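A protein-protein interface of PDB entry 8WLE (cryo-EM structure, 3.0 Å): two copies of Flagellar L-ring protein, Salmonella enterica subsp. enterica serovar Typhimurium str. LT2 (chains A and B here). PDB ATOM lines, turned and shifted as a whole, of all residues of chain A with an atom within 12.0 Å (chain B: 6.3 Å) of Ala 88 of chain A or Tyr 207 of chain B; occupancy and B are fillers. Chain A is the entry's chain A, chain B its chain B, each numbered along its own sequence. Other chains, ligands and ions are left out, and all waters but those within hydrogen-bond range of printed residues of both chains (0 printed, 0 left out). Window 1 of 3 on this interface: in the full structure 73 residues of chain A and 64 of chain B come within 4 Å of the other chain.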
ATOM      1  N   GLN A  83      15.127  10.941  24.635  1.00  0.00           N
ATOM      2  CA  GLN A  83      15.117  12.257  25.269  1.00  0.00           C
ATOM      3  C   GLN A  83      13.846  12.952  24.785  1.00  0.00           C
ATOM      4  O   GLN A  83      13.830  13.601  23.738  1.00  0.00           O
ATOM      5  CB  GLN A  83      16.371  13.056  24.946  1.00  0.00           C
ATOM      6  CG  GLN A  83      16.812  12.997  23.490  1.00  0.00           C
ATOM      7  CD  GLN A  83      18.096  13.759  23.239  1.00  0.00           C
ATOM      8  OE1 GLN A  83      19.175  13.331  23.645  1.00  0.00           O
ATOM      9  NE2 GLN A  83      17.987  14.898  22.569  1.00  0.00           N
ATOM     10  N   GLU A  84      12.785  12.802  25.567  1.00  0.00           N
ATOM     11  CA  GLU A  84      11.493  13.394  25.271  1.00  0.00           C
ATOM     12  C   GLU A  84      11.184  14.438  26.328  1.00  0.00           C
ATOM     13  O   GLU A  84      11.360  14.192  27.522  1.00  0.00           O
ATOM     14  CB  GLU A  84      10.385  12.337  25.245  1.00  0.00           C
ATOM     15  CG  GLU A  84      10.670  11.157  24.339  1.00  0.00           C
ATOM     16  CD  GLU A  84      10.666  11.530  22.872  1.00  0.00           C
ATOM     17  OE1 GLU A  84      10.025  12.538  22.509  1.00  0.00           O
ATOM     18  OE2 GLU A  84      11.307  10.812  22.078  1.00  0.00           O
ATOM     19  N   ASN A  85      10.738  15.607  25.878  1.00  0.00           N
ATOM     20  CA  ASN A  85      10.343  16.685  26.781  1.00  0.00           C
ATOM     21  C   ASN A  85       9.219  17.448  26.084  1.00  0.00           C
ATOM     22  O   ASN A  85       9.471  18.352  25.286  1.00  0.00           O
ATOM     23  CB  ASN A  85      11.511  17.594  27.121  1.00  0.00           C
ATOM     24  CG  ASN A  85      11.965  17.447  28.553  1.00  0.00           C
ATOM     25  OD1 ASN A  85      12.853  16.651  28.855  1.00  0.00           O
ATOM     26  ND2 ASN A  85      11.353  18.214  29.447  1.00  0.00           N
ATOM     27  N   VAL A  86       7.983  17.076  26.397  1.00  0.00           N
ATOM     28  CA  VAL A  86       6.809  17.722  25.829  1.00  0.00           C
ATOM     29  C   VAL A  86       6.076  18.423  26.957  1.00  0.00           C
ATOM     30  O   VAL A  86       5.872  17.839  28.026  1.00  0.00           O
ATOM     31  CB  VAL A  86       5.888  16.720  25.114  1.00  0.00           C
ATOM     32  CG1 VAL A  86       4.675  17.429  24.557  1.00  0.00           C
ATOM     33  CG2 VAL A  86       6.638  16.012  24.006  1.00  0.00           C
ATOM     34  N   SER A  87       5.707  19.679  26.731  1.00  0.00           N
ATOM     35  CA  SER A  87       4.973  20.445  27.731  1.00  0.00           C
ATOM     36  C   SER A  87       4.025  21.378  26.997  1.00  0.00           C
ATOM     37  O   SER A  87       4.467  22.343  26.369  1.00  0.00           O
ATOM     38  CB  SER A  87       5.923  21.222  28.634  1.00  0.00           C
ATOM     39  OG  SER A  87       5.206  21.919  29.642  1.00  0.00           O
ATOM     40  N   ALA A  88       2.733  21.093  27.084  1.00  0.00           N
ATOM     41  CA  ALA A  88       1.701  21.911  26.476  1.00  0.00           C
ATOM     42  C   ALA A  88       0.817  22.487  27.568  1.00  0.00           C
ATOM     43  O   ALA A  88       0.618  21.867  28.612  1.00  0.00           O
ATOM     44  CB  ALA A  88       0.852  21.099  25.496  1.00  0.00           C
ATOM     45  N   SER A  89       0.299  23.686  27.328  1.00  0.00           N
ATOM     46  CA  SER A  89      -0.560  24.332  28.307  1.00  0.00           C
ATOM     47  C   SER A  89      -1.539  25.241  27.588  1.00  0.00           C
ATOM     48  O   SER A  89      -1.304  25.677  26.461  1.00  0.00           O
ATOM     49  CB  SER A  89       0.249  25.135  29.329  1.00  0.00           C
ATOM     50  OG  SER A  89       1.136  24.297  30.046  1.00  0.00           O
ATOM     51  N   LYS A  90      -2.652  25.510  28.260  1.00  0.00           N
ATOM     52  CA  LYS A  90      -3.616  26.488  27.795  1.00  0.00           C
ATOM     53  C   LYS A  90      -4.414  26.965  28.993  1.00  0.00           C
ATOM     54  O   LYS A  90      -4.599  26.229  29.964  1.00  0.00           O
ATOM     55  CB  LYS A  90      -4.551  25.913  26.728  1.00  0.00           C
ATOM     56  CG  LYS A  90      -5.446  24.805  27.225  1.00  0.00           C
ATOM     57  CD  LYS A  90      -6.390  24.341  26.140  1.00  0.00           C
ATOM     58  CE  LYS A  90      -7.282  23.227  26.640  1.00  0.00           C
ATOM     59  NZ  LYS A  90      -8.106  22.652  25.546  1.00  0.00           N
ATOM     60  N   SER A  91      -4.878  28.207  28.919  1.00  0.00           N
ATOM     61  CA  SER A  91      -5.702  28.766  29.977  1.00  0.00           C
ATOM     62  C   SER A  91      -6.535  29.885  29.388  1.00  0.00           C
ATOM     63  O   SER A  91      -6.158  30.504  28.391  1.00  0.00           O
ATOM     64  CB  SER A  91      -4.853  29.275  31.146  1.00  0.00           C
ATOM     65  OG  SER A  91      -3.975  30.299  30.728  1.00  0.00           O
ATOM     66  N   SER A  92      -7.675  30.144  30.022  1.00  0.00           N
ATOM     67  CA  SER A  92      -8.569  31.181  29.537  1.00  0.00           C
ATOM     68  C   SER A  92      -9.473  31.617  30.677  1.00  0.00           C
ATOM     69  O   SER A  92      -9.652  30.897  31.662  1.00  0.00           O
ATOM     70  CB  SER A  92      -9.401  30.698  28.348  1.00  0.00           C
ATOM     71  OG  SER A  92     -10.294  29.676  28.741  1.00  0.00           O
ATOM     72  N   GLY A 136     -10.886  28.667  33.074  1.00  0.00           N
ATOM     73  CA  GLY A 136     -10.583  27.283  32.773  1.00  0.00           C
ATOM     74  C   GLY A 136      -9.168  27.167  32.266  1.00  0.00           C
ATOM     75  O   GLY A 136      -8.493  28.166  32.001  1.00  0.00           O
ATOM     76  N   GLY A 137      -8.729  25.924  32.124  1.00  0.00           N
ATOM     77  CA  GLY A 137      -7.388  25.669  31.656  1.00  0.00           C
ATOM     78  C   GLY A 137      -7.008  24.206  31.690  1.00  0.00           C
ATOM     79  O   GLY A 137      -7.721  23.379  32.262  1.00  0.00           O
ATOM     80  N   ALA A 138      -5.883  23.879  31.065  1.00  0.00           N
ATOM     81  CA  ALA A 138      -5.366  22.522  31.057  1.00  0.00           C
ATOM     82  C   ALA A 138      -3.871  22.586  30.813  1.00  0.00           C
ATOM     83  O   ALA A 138      -3.352  23.589  30.318  1.00  0.00           O
ATOM     84  CB  ALA A 138      -6.045  21.659  29.990  1.00  0.00           C
ATOM     85  N   ASN A 139      -3.182  21.515  31.184  1.00  0.00           N
ATOM     86  CA  ASN A 139      -1.766  21.402  30.879  1.00  0.00           C
ATOM     87  C   ASN A 139      -1.385  19.935  30.894  1.00  0.00           C
ATOM     88  O   ASN A 139      -1.919  19.147  31.675  1.00  0.00           O
ATOM     89  CB  ASN A 139      -0.899  22.193  31.863  1.00  0.00           C
ATOM     90  CG  ASN A 139      -1.111  21.769  33.294  1.00  0.00           C
ATOM     91  OD1 ASN A 139      -1.933  22.343  34.006  1.00  0.00           O
ATOM     92  ND2 ASN A 139      -0.367  20.764  33.731  1.00  0.00           N
ATOM     93  N   ALA A 140      -0.464  19.583  30.009  1.00  0.00           N
ATOM     94  CA  ALA A 140       0.059  18.234  29.922  1.00  0.00           C
ATOM     95  C   ALA A 140       1.570  18.316  29.818  1.00  0.00           C
ATOM     96  O   ALA A 140       2.120  19.268  29.260  1.00  0.00           O
ATOM     97  CB  ALA A 140      -0.516  17.476  28.723  1.00  0.00           C
ATOM     98  N   SER A 141       2.238  17.314  30.372  1.00  0.00           N
ATOM     99  CA  SER A 141       3.686  17.271  30.325  1.00  0.00           C
ATOM    100  C   SER A 141       4.131  15.822  30.353  1.00  0.00           C
ATOM    101  O   SER A 141       3.477  14.961  30.942  1.00  0.00           O
ATOM    102  CB  SER A 141       4.308  18.048  31.488  1.00  0.00           C
ATOM    103  OG  SER A 141       5.719  17.925  31.483  1.00  0.00           O
ATOM    104  N   ASN A 142       5.260  15.564  29.707  1.00  0.00           N
ATOM    105  CA  ASN A 142       5.871  14.251  29.787  1.00  0.00           C
ATOM    106  C   ASN A 142       7.352  14.385  29.492  1.00  0.00           C
ATOM    107  O   ASN A 142       7.778  15.243  28.711  1.00  0.00           O
ATOM    108  CB  ASN A 142       5.217  13.240  28.835  1.00  0.00           C
ATOM    109  CG  ASN A 142       5.620  13.442  27.398  1.00  0.00           C
ATOM    110  OD1 ASN A 142       6.705  13.042  26.982  1.00  0.00           O
ATOM    111  ND2 ASN A 142       4.737  14.050  26.621  1.00  0.00           N
ATOM    112  N   THR A 143       8.126  13.526  30.142  1.00  0.00           N
ATOM    113  CA  THR A 143       9.571  13.522  30.040  1.00  0.00           C
ATOM    114  C   THR A 143      10.038  12.079  29.954  1.00  0.00           C
ATOM    115  O   THR A 143       9.418  11.177  30.517  1.00  0.00           O
ATOM    116  CB  THR A 143      10.214  14.225  31.242  1.00  0.00           C
ATOM    117  OG1 THR A 143       9.574  15.487  31.450  1.00  0.00           O
ATOM    118  CG2 THR A 143      11.691  14.463  31.009  1.00  0.00           C
ATOM    119  N   PHE A 144      11.130  11.872  29.235  1.00  0.00           N
ATOM    120  CA  PHE A 144      11.729  10.553  29.115  1.00  0.00           C
ATOM    121  C   PHE A 144      13.216  10.734  28.879  1.00  0.00           C
ATOM    122  O   PHE A 144      13.619  11.556  28.055  1.00  0.00           O
ATOM    123  CB  PHE A 144      11.106   9.752  27.971  1.00  0.00           C
ATOM    124  CG  PHE A 144      11.067   8.275  28.218  1.00  0.00           C
ATOM    125  CD1 PHE A 144      12.227   7.573  28.488  1.00  0.00           C
ATOM    126  CD2 PHE A 144       9.870   7.587  28.177  1.00  0.00           C
ATOM    127  CE1 PHE A 144      12.193   6.215  28.716  1.00  0.00           C
ATOM    128  CE2 PHE A 144       9.830   6.227  28.402  1.00  0.00           C
ATOM    129  CZ  PHE A 144      10.994   5.540  28.671  1.00  0.00           C
ATOM    130  N   ALA A 203       7.538   7.127  16.566  1.00  0.00           N
ATOM    131  CA  ALA A 203       8.094   6.745  17.854  1.00  0.00           C
ATOM    132  C   ALA A 203       7.020   6.117  18.730  1.00  0.00           C
ATOM    133  O   ALA A 203       6.010   6.747  19.045  1.00  0.00           O
ATOM    134  CB  ALA A 203       8.704   7.959  18.548  1.00  0.00           C
ATOM    135  N   ILE A 205       7.171   4.472  22.357  1.00  0.00           N
ATOM    136  CA  ILE A 205       7.997   4.277  23.542  1.00  0.00           C
ATOM    137  C   ILE A 205       7.108   3.765  24.662  1.00  0.00           C
ATOM    138  O   ILE A 205       6.058   4.351  24.947  1.00  0.00           O
ATOM    139  CB  ILE A 205       8.707   5.576  23.952  1.00  0.00           C
ATOM    140  CG1 ILE A 205       9.178   6.336  22.712  1.00  0.00           C
ATOM    141  CG2 ILE A 205       9.885   5.267  24.855  1.00  0.00           C
ATOM    142  CD1 ILE A 205       9.812   7.668  23.023  1.00  0.00           C
ATOM    143  N   THR B 143       0.180  27.280  25.101  1.00  0.00           N
ATOM    144  CA  THR B 143       1.601  27.078  24.913  1.00  0.00           C
ATOM    145  C   THR B 143       1.831  25.621  24.550  1.00  0.00           C
ATOM    146  O   THR B 143       1.094  24.735  24.984  1.00  0.00           O
ATOM    147  CB  THR B 143       2.385  27.447  26.178  1.00  0.00           C
ATOM    148  OG1 THR B 143       1.960  28.732  26.640  1.00  0.00           O
ATOM    149  CG2 THR B 143       3.873  27.499  25.902  1.00  0.00           C
ATOM    150  N   PHE B 144       2.853  25.385  23.743  1.00  0.00           N
ATOM    151  CA  PHE B 144       3.231  24.035  23.360  1.00  0.00           C
ATOM    152  C   PHE B 144       4.720  24.031  23.070  1.00  0.00           C
ATOM    153  O   PHE B 144       5.222  24.918  22.379  1.00  0.00           O
ATOM    154  CB  PHE B 144       2.453  23.557  22.133  1.00  0.00           C
ATOM    155  CG  PHE B 144       2.190  22.082  22.123  1.00  0.00           C
ATOM    156  CD1 PHE B 144       3.231  21.177  22.195  1.00  0.00           C
ATOM    157  CD2 PHE B 144       0.896  21.601  22.033  1.00  0.00           C
ATOM    158  CE1 PHE B 144       2.990  19.820  22.186  1.00  0.00           C
ATOM    159  CE2 PHE B 144       0.650  20.245  22.021  1.00  0.00           C
ATOM    160  CZ  PHE B 144       1.699  19.353  22.096  1.00  0.00           C
ATOM    161  N   SER B 145       5.417  23.024  23.589  1.00  0.00           N
ATOM    162  CA  SER B 145       6.845  22.887  23.350  1.00  0.00           C
ATOM    163  C   SER B 145       7.185  21.412  23.261  1.00  0.00           C
ATOM    164  O   SER B 145       6.854  20.639  24.163  1.00  0.00           O
ATOM    165  CB  SER B 145       7.662  23.550  24.459  1.00  0.00           C
ATOM    166  OG  SER B 145       7.638  22.769  25.637  1.00  0.00           O
ATOM    167  N   GLU B 176      -0.010   8.244  26.304  1.00  0.00           N
ATOM    168  CA  GLU B 176      -0.156   9.583  25.760  1.00  0.00           C
ATOM    169  C   GLU B 176       0.103   9.550  24.260  1.00  0.00           C
ATOM    170  O   GLU B 176       1.057   8.916  23.798  1.00  0.00           O
ATOM    171  CB  GLU B 176       0.817  10.558  26.421  1.00  0.00           C
ATOM    172  CG  GLU B 176       0.582  10.771  27.898  1.00  0.00           C
ATOM    173  CD  GLU B 176       1.677  11.598  28.535  1.00  0.00           C
ATOM    174  OE1 GLU B 176       2.863  11.341  28.237  1.00  0.00           O
ATOM    175  OE2 GLU B 176       1.355  12.513  29.322  1.00  0.00           O
ATOM    176  N   PHE B 177      -0.742  10.255  23.514  1.00  0.00           N
ATOM    177  CA  PHE B 177      -0.629  10.369  22.069  1.00  0.00           C
ATOM    178  C   PHE B 177      -0.391  11.827  21.715  1.00  0.00           C
ATOM    179  O   PHE B 177      -1.166  12.702  22.122  1.00  0.00           O
ATOM    180  CB  PHE B 177      -1.893   9.873  21.358  1.00  0.00           C
ATOM    181  CG  PHE B 177      -2.422   8.566  21.874  1.00  0.00           C
ATOM    182  CD1 PHE B 177      -3.261   8.526  22.974  1.00  0.00           C
ATOM    183  CD2 PHE B 177      -2.114   7.380  21.237  1.00  0.00           C
ATOM    184  CE1 PHE B 177      -3.755   7.328  23.441  1.00  0.00           C
ATOM    185  CE2 PHE B 177      -2.608   6.179  21.702  1.00  0.00           C
ATOM    186  CZ  PHE B 177      -3.429   6.154  22.803  1.00  0.00           C
ATOM    187  N   ILE B 178       0.672  12.082  20.959  1.00  0.00           N
ATOM    188  CA  ILE B 178       0.961  13.394  20.400  1.00  0.00           C
ATOM    189  C   ILE B 178       0.865  13.248  18.891  1.00  0.00           C
ATOM    190  O   ILE B 178       1.697  12.575  18.273  1.00  0.00           O
ATOM    191  CB  ILE B 178       2.344  13.918  20.809  1.00  0.00           C
ATOM    192  CG1 ILE B 178       2.485  13.969  22.329  1.00  0.00           C
ATOM    193  CG2 ILE B 178       2.581  15.291  20.218  1.00  0.00           C
ATOM    194  CD1 ILE B 178       3.135  12.749  22.938  1.00  0.00           C
ATOM    195  N   ARG B 179      -0.138  13.875  18.295  1.00  0.00           N
ATOM    196  CA  ARG B 179      -0.367  13.797  16.863  1.00  0.00           C
ATOM    197  C   ARG B 179      -0.163  15.166  16.237  1.00  0.00           C
ATOM    198  O   ARG B 179      -0.455  16.196  16.847  1.00  0.00           O
ATOM    199  CB  ARG B 179      -1.774  13.290  16.543  1.00  0.00           C
ATOM    200  CG  ARG B 179      -2.056  11.886  17.028  1.00  0.00           C
ATOM    201  CD  ARG B 179      -3.422  11.424  16.574  1.00  0.00           C
ATOM    202  NE  ARG B 179      -3.795  10.152  17.178  1.00  0.00           N
ATOM    203  CZ  ARG B 179      -4.514  10.035  18.285  1.00  0.00           C
ATOM    204  NH1 ARG B 179      -4.955  11.095  18.938  1.00  0.00           N
ATOM    205  NH2 ARG B 179      -4.801   8.822  18.747  1.00  0.00           N
ATOM    206  N   ILE B 205      -2.445  20.030  15.933  1.00  0.00           N
ATOM    207  CA  ILE B 205      -1.624  19.503  17.014  1.00  0.00           C
ATOM    208  C   ILE B 205      -2.545  18.935  18.080  1.00  0.00           C
ATOM    209  O   ILE B 205      -3.480  19.611  18.525  1.00  0.00           O
ATOM    210  CB  ILE B 205      -0.703  20.585  17.601  1.00  0.00           C
ATOM    211  CG1 ILE B 205      -0.158  21.476  16.486  1.00  0.00           C
ATOM    212  CG2 ILE B 205       0.439  19.944  18.364  1.00  0.00           C
ATOM    213  CD1 ILE B 205       0.688  22.619  16.984  1.00  0.00           C
ATOM    214  N   GLU B 206      -2.287  17.696  18.487  1.00  0.00           N
ATOM    215  CA  GLU B 206      -3.110  16.996  19.458  1.00  0.00           C
ATOM    216  C   GLU B 206      -2.221  16.364  20.515  1.00  0.00           C
ATOM    217  O   GLU B 206      -1.203  15.755  20.190  1.00  0.00           O
ATOM    218  CB  GLU B 206      -3.953  15.924  18.773  1.00  0.00           C
ATOM    219  CG  GLU B 206      -4.998  15.287  19.651  1.00  0.00           C
ATOM    220  CD  GLU B 206      -5.784  14.230  18.915  1.00  0.00           C
ATOM    221  OE1 GLU B 206      -5.334  13.813  17.827  1.00  0.00           O
ATOM    222  OE2 GLU B 206      -6.848  13.817  19.419  1.00  0.00           O
ATOM    223  N   TYR B 207      -2.617  16.499  21.776  1.00  0.00           N
ATOM    224  CA  TYR B 207      -1.871  15.933  22.900  1.00  0.00           C
ATOM    225  C   TYR B 207      -2.902  15.383  23.877  1.00  0.00           C
ATOM    226  O   TYR B 207      -3.444  16.128  24.697  1.00  0.00           O
ATOM    227  CB  TYR B 207      -0.981  16.976  23.565  1.00  0.00           C
ATOM    228  CG  TYR B 207       0.007  16.413  24.564  1.00  0.00           C
ATOM    229  CD1 TYR B 207       0.224  15.049  24.666  1.00  0.00           C
ATOM    230  CD2 TYR B 207       0.722  17.250  25.407  1.00  0.00           C
ATOM    231  CE1 TYR B 207       1.127  14.534  25.572  1.00  0.00           C
ATOM    232  CE2 TYR B 207       1.625  16.744  26.317  1.00  0.00           C
ATOM    233  CZ  TYR B 207       1.821  15.386  26.395  1.00  0.00           C
ATOM    234  OH  TYR B 207       2.722  14.880  27.301  1.00  0.00           O
ATOM    235  N   VAL B 208      -3.163  14.084  23.796  1.00  0.00           N
ATOM    236  CA  VAL B 208      -4.203  13.448  24.583  1.00  0.00           C
ATOM    237  C   VAL B 208      -3.597  12.267  25.330  1.00  0.00           C
ATOM    238  O   VAL B 208      -2.437  11.915  25.138  1.00  0.00           O
ATOM    239  CB  VAL B 208      -5.395  12.998  23.718  1.00  0.00           C
ATOM    240  CG1 VAL B 208      -6.099  14.203  23.123  1.00  0.00           C
ATOM    241  CG2 VAL B 208      -4.921  12.064  22.628  1.00  0.00           C
ATOM    242  N   GLY B 209      -4.405  11.656  26.190  1.00  0.00           N
ATOM    243  CA  GLY B 209      -3.976  10.486  26.926  1.00  0.00           C
ATOM    244  C   GLY B 209      -5.173   9.665  27.347  1.00  0.00           C
ATOM    245  O   GLY B 209      -6.320  10.105  27.249  1.00  0.00           O
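The backbone carbonyl oxygen (O) of Ser 145 of chain B lies within hydrogen-bond range of the backbone NH (N) of Ser 87 of chain A, 3.0 Å away.
The backbone carbonyl oxygen (O) of Ser 89 of chain A sits at hydrogen-bond distance from the backbone NH (N) of Thr 143 of chain B.
OH of Tyr 207 of chain B sits close to ND2 of Asn 142 of chain A, 2.3 Å away.
The backbone carbonyl oxygen (O) of Val 86 of chain A sits close to the side-chain hydroxyl (OG) of Ser 141 of chain A (3.5 Å).
N of Asn 142 of chain A is in hydrogen-bond range of O of Val 86 of chain A (2.9 Å).
N of Ala 140 of chain A is in hydrogen-bond range of O of Ala 88 of chain A (2.9 Å).
OH of Tyr 207 of chain B sits at hydrogen-bond distance from OE2 of Glu 176 of chain B (3.4 Å).
Among the printed residues, pairs that only touch across the chains: Asn 142 of chain A with Glu 176 of chain B (3.1 Å), Ala 88 of chain A with Thr 143 of chain B (3.3 Å), Ala 140 of chain A with Tyr 207 of chain B (3.3 Å), Val 86 of chain A with Ser 145 of chain B (3.4 Å), Ser 141 of chain A with Tyr 207 of chain B (3.5 Å), Ala 88 of chain A with Phe 144 of chain B (3.5 Å), Val 86 of chain A with Tyr 207 of chain B (3.6 Å), Ser 141 of chain A with Glu 176 of chain B (3.6 Å), Asn 85 of chain A with Ser 145 of chain B (3.7 Å), Ser 87 of chain A with Phe 144 of chain B (3.7 Å), Val 86 of chain A with Phe 144 of chain B (3.8 Å) and Ala 88 of chain A with Tyr 207 of chain B (3.9 Å).
Of the printed residues of chain B, Asn 85 of chain A touches Ser 145.
Of chain B, only Thr 143, Phe 144 and Tyr 207 come within 4 Å of Ala 88 of chain A.
Of the printed residues of chain B, Ser 89 of chain A touches Thr 143.
Ser 92 of chain A touches none of the printed residues of chain B.
Printed residues of chain B within 4 Å of Asn 142 of chain A: Glu 176 and Tyr 207.
Of chain A, only Ala 88 and Ser 89 come within 4 Å of Thr 143 of chain B.
Phe 144 of chain B touches just these residues of chain A: Val 86, Ser 87 and Ala 88.
Ser 145 of chain B touches three residues of chain A.
Glu 176 of chain B touches just these residues of chain A: Ser 141 and Asn 142.
Of chain A, only Val 86 (3.6 Å), Ala 88 (3.9 Å), Ala 140 (3.3 Å), Ser 141 (3.5 Å) and Asn 142 (2.3 Å) come within 4 Å of Tyr 207 of chain B.
No residue of chain A comes within 4 Å of Gly 209 of chain B.
The nearest residue of chain A that does not touch Tyr 207 of chain B is Ser 87 of chain A (5.0 Å).
Of the 12 printed residues of chain B, 5 touch a printed residue of chain A.
Printed residues of chain B that touch a printed residue of chain A: Thr 143, Phe 144, Ser 145, Glu 176 and Tyr 207.
Of the 21 printed residues of chain A, 8 touch a printed residue of chain B.
Hydrophobic or aromatic side chains of chain A within 4 Å of the printed part of chain B: Val 86, Ala 88 and Ala 140.
Positions printed for both chains: 143, 144 and 205.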
